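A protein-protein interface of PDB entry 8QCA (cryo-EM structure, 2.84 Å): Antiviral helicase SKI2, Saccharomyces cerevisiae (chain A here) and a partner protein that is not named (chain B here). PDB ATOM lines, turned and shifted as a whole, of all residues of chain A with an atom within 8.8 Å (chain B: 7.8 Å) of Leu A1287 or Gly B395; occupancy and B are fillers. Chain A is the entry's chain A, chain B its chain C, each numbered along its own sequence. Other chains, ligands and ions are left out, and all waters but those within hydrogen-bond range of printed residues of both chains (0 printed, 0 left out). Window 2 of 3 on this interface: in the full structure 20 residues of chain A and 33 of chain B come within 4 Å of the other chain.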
ATOM      1  N   SER A 385     -24.645  27.927   3.517  1.00  0.00           N
ATOM      2  CA  SER A 385     -24.925  26.495   3.478  1.00  0.00           C
ATOM      3  C   SER A 385     -25.376  25.975   4.837  1.00  0.00           C
ATOM      4  O   SER A 385     -26.334  25.200   4.922  1.00  0.00           O
ATOM      5  CB  SER A 385     -23.692  25.734   2.994  1.00  0.00           C
ATOM      6  OG  SER A 385     -23.479  25.937   1.609  1.00  0.00           O
ATOM      7  N   ASN A 386     -24.699  26.388   5.910  1.00  0.00           N
ATOM      8  CA  ASN A 386     -25.071  25.926   7.244  1.00  0.00           C
ATOM      9  C   ASN A 386     -26.453  26.432   7.642  1.00  0.00           C
ATOM     10  O   ASN A 386     -27.258  25.685   8.218  1.00  0.00           O
ATOM     11  CB  ASN A 386     -24.020  26.377   8.256  1.00  0.00           C
ATOM     12  CG  ASN A 386     -22.625  25.923   7.884  1.00  0.00           C
ATOM     13  OD1 ASN A 386     -22.420  24.782   7.473  1.00  0.00           O
ATOM     14  ND2 ASN A 386     -21.656  26.818   8.023  1.00  0.00           N
ATOM     15  N   GLN A 387     -26.742  27.701   7.347  1.00  0.00           N
ATOM     16  CA  GLN A 387     -28.054  28.256   7.659  1.00  0.00           C
ATOM     17  C   GLN A 387     -29.152  27.534   6.892  1.00  0.00           C
ATOM     18  O   GLN A 387     -30.210  27.227   7.453  1.00  0.00           O
ATOM     19  CB  GLN A 387     -28.078  29.748   7.346  1.00  0.00           C
ATOM     20  CG  GLN A 387     -26.983  30.536   8.026  1.00  0.00           C
ATOM     21  CD  GLN A 387     -27.340  31.995   8.191  1.00  0.00           C
ATOM     22  OE1 GLN A 387     -26.536  32.877   7.896  1.00  0.00           O
ATOM     23  NE2 GLN A 387     -28.556  32.258   8.656  1.00  0.00           N
ATOM     24  N   PHE A 389     -28.994  24.477   5.752  1.00  0.00           N
ATOM     25  CA  PHE A 389     -29.078  23.134   6.311  1.00  0.00           C
ATOM     26  C   PHE A 389     -29.951  23.117   7.558  1.00  0.00           C
ATOM     27  O   PHE A 389     -30.828  22.260   7.705  1.00  0.00           O
ATOM     28  CB  PHE A 389     -27.673  22.616   6.621  1.00  0.00           C
ATOM     29  CG  PHE A 389     -27.647  21.233   7.199  1.00  0.00           C
ATOM     30  CD1 PHE A 389     -27.914  20.132   6.407  1.00  0.00           C
ATOM     31  CD2 PHE A 389     -27.345  21.033   8.534  1.00  0.00           C
ATOM     32  CE1 PHE A 389     -27.888  18.860   6.936  1.00  0.00           C
ATOM     33  CE2 PHE A 389     -27.316  19.762   9.067  1.00  0.00           C
ATOM     34  CZ  PHE A 389     -27.588  18.675   8.266  1.00  0.00           C
ATOM     35  N   ARG A 390     -29.739  24.078   8.461  1.00  0.00           N
ATOM     36  CA  ARG A 390     -30.569  24.155   9.661  1.00  0.00           C
ATOM     37  C   ARG A 390     -32.023  24.458   9.313  1.00  0.00           C
ATOM     38  O   ARG A 390     -32.946  23.871   9.896  1.00  0.00           O
ATOM     39  CB  ARG A 390     -30.007  25.209  10.617  1.00  0.00           C
ATOM     40  CG  ARG A 390     -30.759  25.353  11.937  1.00  0.00           C
ATOM     41  CD  ARG A 390     -31.107  24.011  12.571  1.00  0.00           C
ATOM     42  NE  ARG A 390     -29.955  23.127  12.690  1.00  0.00           N
ATOM     43  CZ  ARG A 390     -30.028  21.846  13.028  1.00  0.00           C
ATOM     44  NH1 ARG A 390     -31.187  21.269  13.297  1.00  0.00           N
ATOM     45  NH2 ARG A 390     -28.912  21.126  13.096  1.00  0.00           N
ATOM     46  N   LYS A 393     -33.568  21.346   7.889  1.00  0.00           N
ATOM     47  CA  LYS A 393     -33.734  20.378   8.967  1.00  0.00           C
ATOM     48  C   LYS A 393     -34.976  20.685   9.789  1.00  0.00           C
ATOM     49  O   LYS A 393     -35.744  19.777  10.129  1.00  0.00           O
ATOM     50  CB  LYS A 393     -32.495  20.369   9.864  1.00  0.00           C
ATOM     51  CG  LYS A 393     -31.482  19.285   9.546  1.00  0.00           C
ATOM     52  CD  LYS A 393     -32.032  17.909   9.871  1.00  0.00           C
ATOM     53  CE  LYS A 393     -31.256  16.816   9.159  1.00  0.00           C
ATOM     54  NZ  LYS A 393     -32.059  15.571   9.010  1.00  0.00           N
ATOM     55  N   ILE A 401     -31.966  15.315   4.943  1.00  0.00           N
ATOM     56  CA  ILE A 401     -31.109  16.201   4.171  1.00  0.00           C
ATOM     57  C   ILE A 401     -29.667  15.996   4.612  1.00  0.00           C
ATOM     58  O   ILE A 401     -29.395  15.547   5.730  1.00  0.00           O
ATOM     59  CB  ILE A 401     -31.513  17.682   4.321  1.00  0.00           C
ATOM     60  CG1 ILE A 401     -31.365  18.124   5.771  1.00  0.00           C
ATOM     61  CG2 ILE A 401     -32.948  17.892   3.870  1.00  0.00           C
ATOM     62  CD1 ILE A 401     -31.513  19.599   5.952  1.00  0.00           C
ATOM     63  N   GLY A 402     -28.737  16.333   3.716  1.00  0.00           N
ATOM     64  CA  GLY A 402     -27.327  16.212   4.001  1.00  0.00           C
ATOM     65  C   GLY A 402     -26.577  17.465   3.584  1.00  0.00           C
ATOM     66  O   GLY A 402     -27.106  18.331   2.885  1.00  0.00           O
ATOM     67  N   LEU A 403     -25.328  17.543   4.033  1.00  0.00           N
ATOM     68  CA  LEU A 403     -24.455  18.668   3.730  1.00  0.00           C
ATOM     69  C   LEU A 403     -23.116  18.136   3.248  1.00  0.00           C
ATOM     70  O   LEU A 403     -22.521  17.270   3.895  1.00  0.00           O
ATOM     71  CB  LEU A 403     -24.264  19.565   4.957  1.00  0.00           C
ATOM     72  CG  LEU A 403     -23.415  20.822   4.767  1.00  0.00           C
ATOM     73  CD1 LEU A 403     -24.222  21.920   4.103  1.00  0.00           C
ATOM     74  CD2 LEU A 403     -22.861  21.292   6.099  1.00  0.00           C
ATOM     75  N   THR A 405     -19.298  19.330   2.169  1.00  0.00           N
ATOM     76  CA  THR A 405     -18.277  20.365   2.203  1.00  0.00           C
ATOM     77  C   THR A 405     -17.000  19.820   1.566  1.00  0.00           C
ATOM     78  O   THR A 405     -16.982  18.725   0.998  1.00  0.00           O
ATOM     79  CB  THR A 405     -18.035  20.845   3.635  1.00  0.00           C
ATOM     80  OG1 THR A 405     -17.938  19.715   4.510  1.00  0.00           O
ATOM     81  CG2 THR A 405     -19.172  21.740   4.098  1.00  0.00           C
ATOM     82  N   VAL A 408     -15.934  17.415   5.026  1.00  0.00           N
ATOM     83  CA  VAL A 408     -16.923  16.760   5.875  1.00  0.00           C
ATOM     84  C   VAL A 408     -18.149  16.405   5.049  1.00  0.00           C
ATOM     85  O   VAL A 408     -18.639  17.219   4.255  1.00  0.00           O
ATOM     86  CB  VAL A 408     -17.307  17.654   7.070  1.00  0.00           C
ATOM     87  N   GLN A 409     -18.646  15.185   5.234  1.00  0.00           N
ATOM     88  CA  GLN A 409     -19.864  14.711   4.590  1.00  0.00           C
ATOM     89  C   GLN A 409     -20.846  14.286   5.669  1.00  0.00           C
ATOM     90  O   GLN A 409     -20.521  13.441   6.509  1.00  0.00           O
ATOM     91  CB  GLN A 409     -19.570  13.545   3.643  1.00  0.00           C
ATOM     92  CG  GLN A 409     -18.554  13.859   2.564  1.00  0.00           C
ATOM     93  CD  GLN A 409     -18.166  12.636   1.760  1.00  0.00           C
ATOM     94  OE1 GLN A 409     -18.727  11.556   1.943  1.00  0.00           O
ATOM     95  NE2 GLN A 409     -17.202  12.799   0.863  1.00  0.00           N
ATOM     96  N   ILE A 410     -22.042  14.869   5.647  1.00  0.00           N
ATOM     97  CA  ILE A 410     -23.095  14.556   6.605  1.00  0.00           C
ATOM     98  C   ILE A 410     -24.261  13.959   5.834  1.00  0.00           C
ATOM     99  O   ILE A 410     -24.790  14.595   4.915  1.00  0.00           O
ATOM    100  CB  ILE A 410     -23.537  15.798   7.394  1.00  0.00           C
ATOM    101  CG1 ILE A 410     -22.355  16.386   8.162  1.00  0.00           C
ATOM    102  CG2 ILE A 410     -24.671  15.451   8.342  1.00  0.00           C
ATOM    103  CD1 ILE A 410     -22.718  17.580   9.002  1.00  0.00           C
ATOM    104  N   ASN A 411     -24.660  12.742   6.211  1.00  0.00           N
ATOM    105  CA  ASN A 411     -25.718  11.992   5.541  1.00  0.00           C
ATOM    106  C   ASN A 411     -25.474  11.937   4.037  1.00  0.00           C
ATOM    107  O   ASN A 411     -26.225  12.550   3.270  1.00  0.00           O
ATOM    108  CB  ASN A 411     -27.087  12.609   5.829  1.00  0.00           C
ATOM    109  CG  ASN A 411     -27.382  12.709   7.308  1.00  0.00           C
ATOM    110  OD1 ASN A 411     -26.803  11.988   8.118  1.00  0.00           O
ATOM    111  ND2 ASN A 411     -28.287  13.609   7.671  1.00  0.00           N
ATOM    112  N   ARG A 670     -17.855  23.279  23.244  1.00  0.00           N
ATOM    113  CA  ARG A 670     -17.057  22.421  22.382  1.00  0.00           C
ATOM    114  C   ARG A 670     -15.614  22.886  22.252  1.00  0.00           C
ATOM    115  O   ARG A 670     -14.809  22.192  21.622  1.00  0.00           O
ATOM    116  CB  ARG A 670     -17.686  22.334  20.989  1.00  0.00           C
ATOM    117  CG  ARG A 670     -17.862  23.677  20.306  1.00  0.00           C
ATOM    118  CD  ARG A 670     -18.716  23.554  19.059  1.00  0.00           C
ATOM    119  NE  ARG A 670     -20.133  23.461  19.385  1.00  0.00           N
ATOM    120  CZ  ARG A 670     -21.079  23.115  18.523  1.00  0.00           C
ATOM    121  NH1 ARG A 670     -20.795  22.832  17.263  1.00  0.00           N
ATOM    122  NH2 ARG A 670     -22.340  23.048  18.937  1.00  0.00           N
ATOM    123  N   GLU A 705     -21.739  32.953  13.908  1.00  0.00           N
ATOM    124  CA  GLU A 705     -22.907  32.084  14.024  1.00  0.00           C
ATOM    125  C   GLU A 705     -23.688  32.376  15.299  1.00  0.00           C
ATOM    126  O   GLU A 705     -24.923  32.423  15.282  1.00  0.00           O
ATOM    127  CB  GLU A 705     -22.479  30.617  13.988  1.00  0.00           C
ATOM    128  CG  GLU A 705     -22.059  30.122  12.618  1.00  0.00           C
ATOM    129  CD  GLU A 705     -21.235  28.851  12.688  1.00  0.00           C
ATOM    130  OE1 GLU A 705     -20.808  28.479  13.801  1.00  0.00           O
ATOM    131  OE2 GLU A 705     -21.015  28.224  11.631  1.00  0.00           O
ATOM    132  N   ILE A 709     -27.565  33.683  15.345  1.00  0.00           N
ATOM    133  CA  ILE A 709     -28.613  32.932  16.031  1.00  0.00           C
ATOM    134  C   ILE A 709     -29.283  33.792  17.096  1.00  0.00           C
ATOM    135  O   ILE A 709     -30.513  33.796  17.229  1.00  0.00           O
ATOM    136  CB  ILE A 709     -28.043  31.632  16.625  1.00  0.00           C
ATOM    137  CG1 ILE A 709     -27.569  30.700  15.511  1.00  0.00           C
ATOM    138  CG2 ILE A 709     -29.086  30.934  17.472  1.00  0.00           C
ATOM    139  CD1 ILE A 709     -26.840  29.476  16.012  1.00  0.00           C
ATOM    140  N   ALA A1282     -13.470  23.930  14.213  1.00  0.00           N
ATOM    141  CA  ALA A1282     -14.565  23.615  15.117  1.00  0.00           C
ATOM    142  C   ALA A1282     -15.854  23.388  14.338  1.00  0.00           C
ATOM    143  O   ALA A1282     -16.042  23.914  13.238  1.00  0.00           O
ATOM    144  CB  ALA A1282     -14.763  24.737  16.136  1.00  0.00           C
ATOM    145  N   ALA A1283     -16.746  22.595  14.924  1.00  0.00           N
ATOM    146  CA  ALA A1283     -18.016  22.294  14.280  1.00  0.00           C
ATOM    147  C   ALA A1283     -18.932  23.511  14.297  1.00  0.00           C
ATOM    148  O   ALA A1283     -18.929  24.311  15.236  1.00  0.00           O
ATOM    149  CB  ALA A1283     -18.698  21.114  14.970  1.00  0.00           C
ATOM    150  N   SER A1284     -19.726  23.644  13.238  1.00  0.00           N
ATOM    151  CA  SER A1284     -20.636  24.770  13.115  1.00  0.00           C
ATOM    152  C   SER A1284     -21.741  24.695  14.164  1.00  0.00           C
ATOM    153  O   SER A1284     -22.155  23.614  14.588  1.00  0.00           O
ATOM    154  CB  SER A1284     -21.248  24.809  11.715  1.00  0.00           C
ATOM    155  OG  SER A1284     -22.256  25.798  11.626  1.00  0.00           O
ATOM    156  N   LEU A1285     -22.216  25.869  14.584  1.00  0.00           N
ATOM    157  CA  LEU A1285     -23.301  25.938  15.552  1.00  0.00           C
ATOM    158  C   LEU A1285     -24.645  25.540  14.959  1.00  0.00           C
ATOM    159  O   LEU A1285     -25.610  25.378  15.712  1.00  0.00           O
ATOM    160  CB  LEU A1285     -23.397  27.348  16.139  1.00  0.00           C
ATOM    161  CG  LEU A1285     -22.316  27.765  17.139  1.00  0.00           C
ATOM    162  CD1 LEU A1285     -22.791  28.945  17.965  1.00  0.00           C
ATOM    163  CD2 LEU A1285     -21.928  26.605  18.037  1.00  0.00           C
ATOM    164  N   TYR A1286     -24.730  25.387  13.641  1.00  0.00           N
ATOM    165  CA  TYR A1286     -25.943  24.932  12.977  1.00  0.00           C
ATOM    166  C   TYR A1286     -25.979  23.423  12.788  1.00  0.00           C
ATOM    167  O   TYR A1286     -26.958  22.904  12.243  1.00  0.00           O
ATOM    168  CB  TYR A1286     -26.087  25.619  11.618  1.00  0.00           C
ATOM    169  CG  TYR A1286     -26.263  27.117  11.694  1.00  0.00           C
ATOM    170  CD1 TYR A1286     -27.458  27.675  12.121  1.00  0.00           C
ATOM    171  CD2 TYR A1286     -25.235  27.973  11.331  1.00  0.00           C
ATOM    172  CE1 TYR A1286     -27.623  29.042  12.189  1.00  0.00           C
ATOM    173  CE2 TYR A1286     -25.390  29.341  11.396  1.00  0.00           C
ATOM    174  CZ  TYR A1286     -26.586  29.870  11.824  1.00  0.00           C
ATOM    175  OH  TYR A1286     -26.744  31.235  11.889  1.00  0.00           O
ATOM    176  N   LEU A1287     -24.942  22.711  13.218  1.00  0.00           N
ATOM    177  CA  LEU A1287     -24.876  21.264  13.066  1.00  0.00           C
ATOM    178  C   LEU A1287     -25.305  20.559  14.348  1.00  0.00           C
ATOM    179  O   LEU A1287     -25.222  21.122  15.440  1.00  0.00           O
ATOM    180  CB  LEU A1287     -23.460  20.830  12.680  1.00  0.00           C
ATOM    181  CG  LEU A1287     -23.111  20.709  11.194  1.00  0.00           C
ATOM    182  CD1 LEU A1287     -23.487  21.965  10.426  1.00  0.00           C
ATOM    183  CD2 LEU A1287     -21.631  20.415  11.036  1.00  0.00           C
ATOM    184  OXT LEU A1287     -25.742  19.409  14.324  1.00  0.00           O
ATOM    185  N   VAL B   4     -17.921  14.170  11.991  1.00  0.00           N
ATOM    186  CA  VAL B   4     -17.907  15.306  12.904  1.00  0.00           C
ATOM    187  C   VAL B   4     -18.452  14.853  14.251  1.00  0.00           C
ATOM    188  O   VAL B   4     -19.543  14.276  14.322  1.00  0.00           O
ATOM    189  CB  VAL B   4     -18.723  16.490  12.353  1.00  0.00           C
ATOM    190  CG1 VAL B   4     -18.715  17.644  13.339  1.00  0.00           C
ATOM    191  CG2 VAL B   4     -18.171  16.933  11.011  1.00  0.00           C
ATOM    192  N   ILE B   6     -19.096  16.286  18.284  1.00  0.00           N
ATOM    193  CA  ILE B   6     -19.222  17.473  19.119  1.00  0.00           C
ATOM    194  C   ILE B   6     -19.356  17.033  20.569  1.00  0.00           C
ATOM    195  O   ILE B   6     -20.181  16.169  20.887  1.00  0.00           O
ATOM    196  CB  ILE B   6     -20.428  18.334  18.701  1.00  0.00           C
ATOM    197  CG1 ILE B   6     -20.418  18.567  17.188  1.00  0.00           C
ATOM    198  CG2 ILE B   6     -20.423  19.653  19.452  1.00  0.00           C
ATOM    199  CD1 ILE B   6     -21.768  18.924  16.615  1.00  0.00           C
ATOM    200  N   MET B 371     -28.123  17.678  25.014  1.00  0.00           N
ATOM    201  CA  MET B 371     -27.930  18.814  24.116  1.00  0.00           C
ATOM    202  C   MET B 371     -27.880  18.324  22.671  1.00  0.00           C
ATOM    203  O   MET B 371     -26.819  18.171  22.061  1.00  0.00           O
ATOM    204  CB  MET B 371     -26.662  19.575  24.485  1.00  0.00           C
ATOM    205  N   GLY B 372     -29.063  18.072  22.114  1.00  0.00           N
ATOM    206  CA  GLY B 372     -29.194  17.717  20.717  1.00  0.00           C
ATOM    207  C   GLY B 372     -28.923  16.269  20.380  1.00  0.00           C
ATOM    208  O   GLY B 372     -29.028  15.898  19.204  1.00  0.00           O
ATOM    209  N   ALA B 373     -28.582  15.438  21.362  1.00  0.00           N
ATOM    210  CA  ALA B 373     -28.301  14.023  21.124  1.00  0.00           C
ATOM    211  C   ALA B 373     -29.576  13.234  21.384  1.00  0.00           C
ATOM    212  O   ALA B 373     -29.808  12.730  22.483  1.00  0.00           O
ATOM    213  CB  ALA B 373     -27.152  13.546  22.003  1.00  0.00           C
ATOM    214  N   ASP B 374     -30.421  13.129  20.360  1.00  0.00           N
ATOM    215  CA  ASP B 374     -31.673  12.397  20.495  1.00  0.00           C
ATOM    216  C   ASP B 374     -31.851  11.390  19.366  1.00  0.00           C
ATOM    217  O   ASP B 374     -32.472  10.338  19.558  1.00  0.00           O
ATOM    218  CB  ASP B 374     -32.859  13.365  20.523  1.00  0.00           C
ATOM    219  CG  ASP B 374     -32.754  14.386  21.637  1.00  0.00           C
ATOM    220  OD1 ASP B 374     -33.123  14.056  22.783  1.00  0.00           O
ATOM    221  OD2 ASP B 374     -32.305  15.519  21.366  1.00  0.00           O
ATOM    222  N   LEU B 375     -31.309  11.697  18.186  1.00  0.00           N
ATOM    223  CA  LEU B 375     -31.550  10.885  17.001  1.00  0.00           C
ATOM    224  C   LEU B 375     -30.269  10.413  16.322  1.00  0.00           C
ATOM    225  O   LEU B 375     -30.327   9.959  15.174  1.00  0.00           O
ATOM    226  CB  LEU B 375     -32.411  11.657  15.993  1.00  0.00           C
ATOM    227  N   ASN B 376     -29.121  10.504  16.987  1.00  0.00           N
ATOM    228  CA  ASN B 376     -27.865  10.066  16.398  1.00  0.00           C
ATOM    229  C   ASN B 376     -27.029   9.346  17.446  1.00  0.00           C
ATOM    230  O   ASN B 376     -27.266   9.453  18.652  1.00  0.00           O
ATOM    231  CB  ASN B 376     -27.084  11.239  15.795  1.00  0.00           C
ATOM    232  CG  ASN B 376     -26.400  10.870  14.493  1.00  0.00           C
ATOM    233  OD1 ASN B 376     -26.129   9.699  14.232  1.00  0.00           O
ATOM    234  ND2 ASN B 376     -26.118  11.870  13.669  1.00  0.00           N
ATOM    235  N   GLU B 377     -26.039   8.602  16.960  1.00  0.00           N
ATOM    236  CA  GLU B 377     -25.183   7.792  17.809  1.00  0.00           C
ATOM    237  C   GLU B 377     -24.276   8.681  18.660  1.00  0.00           C
ATOM    238  O   GLU B 377     -23.925   9.801  18.282  1.00  0.00           O
ATOM    239  CB  GLU B 377     -24.356   6.837  16.945  1.00  0.00           C
ATOM    240  CG  GLU B 377     -23.476   5.865  17.706  1.00  0.00           C
ATOM    241  CD  GLU B 377     -23.391   4.514  17.030  1.00  0.00           C
ATOM    242  OE1 GLU B 377     -23.308   4.476  15.785  1.00  0.00           O
ATOM    243  OE2 GLU B 377     -23.414   3.488  17.742  1.00  0.00           O
ATOM    244  N   ARG B 392     -21.233  13.399  20.592  1.00  0.00           N
ATOM    245  CA  ARG B 392     -22.348  13.043  19.727  1.00  0.00           C
ATOM    246  C   ARG B 392     -21.959  13.270  18.275  1.00  0.00           C
ATOM    247  O   ARG B 392     -21.188  14.182  17.961  1.00  0.00           O
ATOM    248  CB  ARG B 392     -23.609  13.849  20.059  1.00  0.00           C
ATOM    249  CG  ARG B 392     -23.518  15.328  19.738  1.00  0.00           C
ATOM    250  CD  ARG B 392     -24.851  16.016  19.971  1.00  0.00           C
ATOM    251  NE  ARG B 392     -24.772  17.456  19.759  1.00  0.00           N
ATOM    252  CZ  ARG B 392     -24.932  18.049  18.585  1.00  0.00           C
ATOM    253  NH1 ARG B 392     -25.179  17.355  17.488  1.00  0.00           N
ATOM    254  NH2 ARG B 392     -24.842  19.374  18.512  1.00  0.00           N
ATOM    255  N   GLU B 393     -22.493  12.433  17.392  1.00  0.00           N
ATOM    256  CA  GLU B 393     -22.226  12.559  15.967  1.00  0.00           C
ATOM    257  C   GLU B 393     -23.132  13.623  15.362  1.00  0.00           C
ATOM    258  O   GLU B 393     -24.345  13.625  15.599  1.00  0.00           O
ATOM    259  CB  GLU B 393     -22.435  11.218  15.268  1.00  0.00           C
ATOM    260  CG  GLU B 393     -22.030  11.210  13.809  1.00  0.00           C
ATOM    261  CD  GLU B 393     -21.840   9.809  13.268  1.00  0.00           C
ATOM    262  OE1 GLU B 393     -21.540   8.899  14.069  1.00  0.00           O
ATOM    263  OE2 GLU B 393     -21.998   9.615  12.045  1.00  0.00           O
ATOM    264  N   ALA B 394     -22.541  14.529  14.588  1.00  0.00           N
ATOM    265  CA  ALA B 394     -23.298  15.624  14.000  1.00  0.00           C
ATOM    266  C   ALA B 394     -24.325  15.104  13.001  1.00  0.00           C
ATOM    267  O   ALA B 394     -24.111  14.099  12.317  1.00  0.00           O
ATOM    268  CB  ALA B 394     -22.358  16.614  13.314  1.00  0.00           C
ATOM    269  N   GLY B 395     -25.454  15.803  12.924  1.00  0.00           N
ATOM    270  CA  GLY B 395     -26.516  15.423  12.015  1.00  0.00           C
ATOM    271  C   GLY B 395     -27.524  14.482  12.638  1.00  0.00           C
ATOM    272  O   GLY B 395     -27.725  14.493  13.856  1.00  0.00           O
ATOM    273  N   GLY B 396     -28.166  13.661  11.811  1.00  0.00           N
ATOM    274  CA  GLY B 396     -29.152  12.718  12.298  1.00  0.00           C
ATOM    275  C   GLY B 396     -29.192  11.438  11.491  1.00  0.00           C
ATOM    276  O   GLY B 396     -28.340  11.217  10.625  1.00  0.00           O
ATOM    277  N   LYS B 397     -30.174  10.586  11.766  1.00  0.00           N
ATOM    278  CA  LYS B 397     -30.315   9.325  11.050  1.00  0.00           C
ATOM    279  C   LYS B 397     -31.744   8.800  11.138  1.00  0.00           C
ATOM    280  O   LYS B 397     -32.414   8.958  12.159  1.00  0.00           O
ATOM    281  CB  LYS B 397     -29.338   8.282  11.600  1.00  0.00           C
ATOM    282  OXT LYS B 397     -32.260   8.205  10.192  1.00  0.00           O
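The chain-end carboxylate of Leu A1287 is in salt-bridge range of the guanidinium group of Arg B392 (3.6 Å). The side-chain amide oxygen (OD1) of Asn A411 sits close to the backbone carbonyl oxygen (O) of Gly B396.
Printed residues of chain A that touch a printed residue of chain B: Asn A411, Arg A670, Ala A1283 and Leu A1287. Hydrophobic or aromatic side chains of chain A within 4 Å of the printed part of chain B: Ala A1283.
Of the printed residues of chain B, Arg A670 touches Ile B6 (3.6 Å). Leu A1287 touches just these residues of chain B: Arg B392 (3.6 Å) and Gly B395 (3.9 Å). Of the printed residues of chain A, Ile B6 touches Arg A670 and Ala A1283. Glu B393 touches none of the printed residues of chain A. No residue of chain A comes within 4 Å of Ala B394. Of chain A, only Leu A1287 (3.9 Å) comes within 4 Å of Gly B395. The nearest residue of chain A that does not touch Gly B395 is Ile A410 (4.1 Å).
The guanidinium group (NE) of Arg B392 sits at hydrogen-bond distance from the backbone carbonyl oxygen (O) of Met B371 (3.2 Å). The backbone carbonyl oxygen (O) of Ile B6 lies within hydrogen-bond range of the backbone NH (N) of Arg B392, at 3.0 Å. The side-chain amide nitrogen (ND2) of Asn B376 lies close to the backbone NH (N) of Gly B396, 3.3 Å away. NH1 of Arg A670 lies within hydrogen-bond range of O of Ser A1284 (3.1 Å). ND2 of Asn A411 is in hydrogen-bond range of O of Ile A401 (3.0 Å). The backbone carbonyl oxygen (O) of Val B4 sits at hydrogen-bond distance from the backbone NH (N) of Ala B394 (3.0 Å).
Among the printed residues, merely in contact across the chains: Arg A670 with Ile B6 (3.6 Å), Ala A1283 with Ile B6 (3.8 Å), Ala A1283 with Val B4 (3.8 Å) and Leu A1287 with Gly B395 (3.9 Å).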
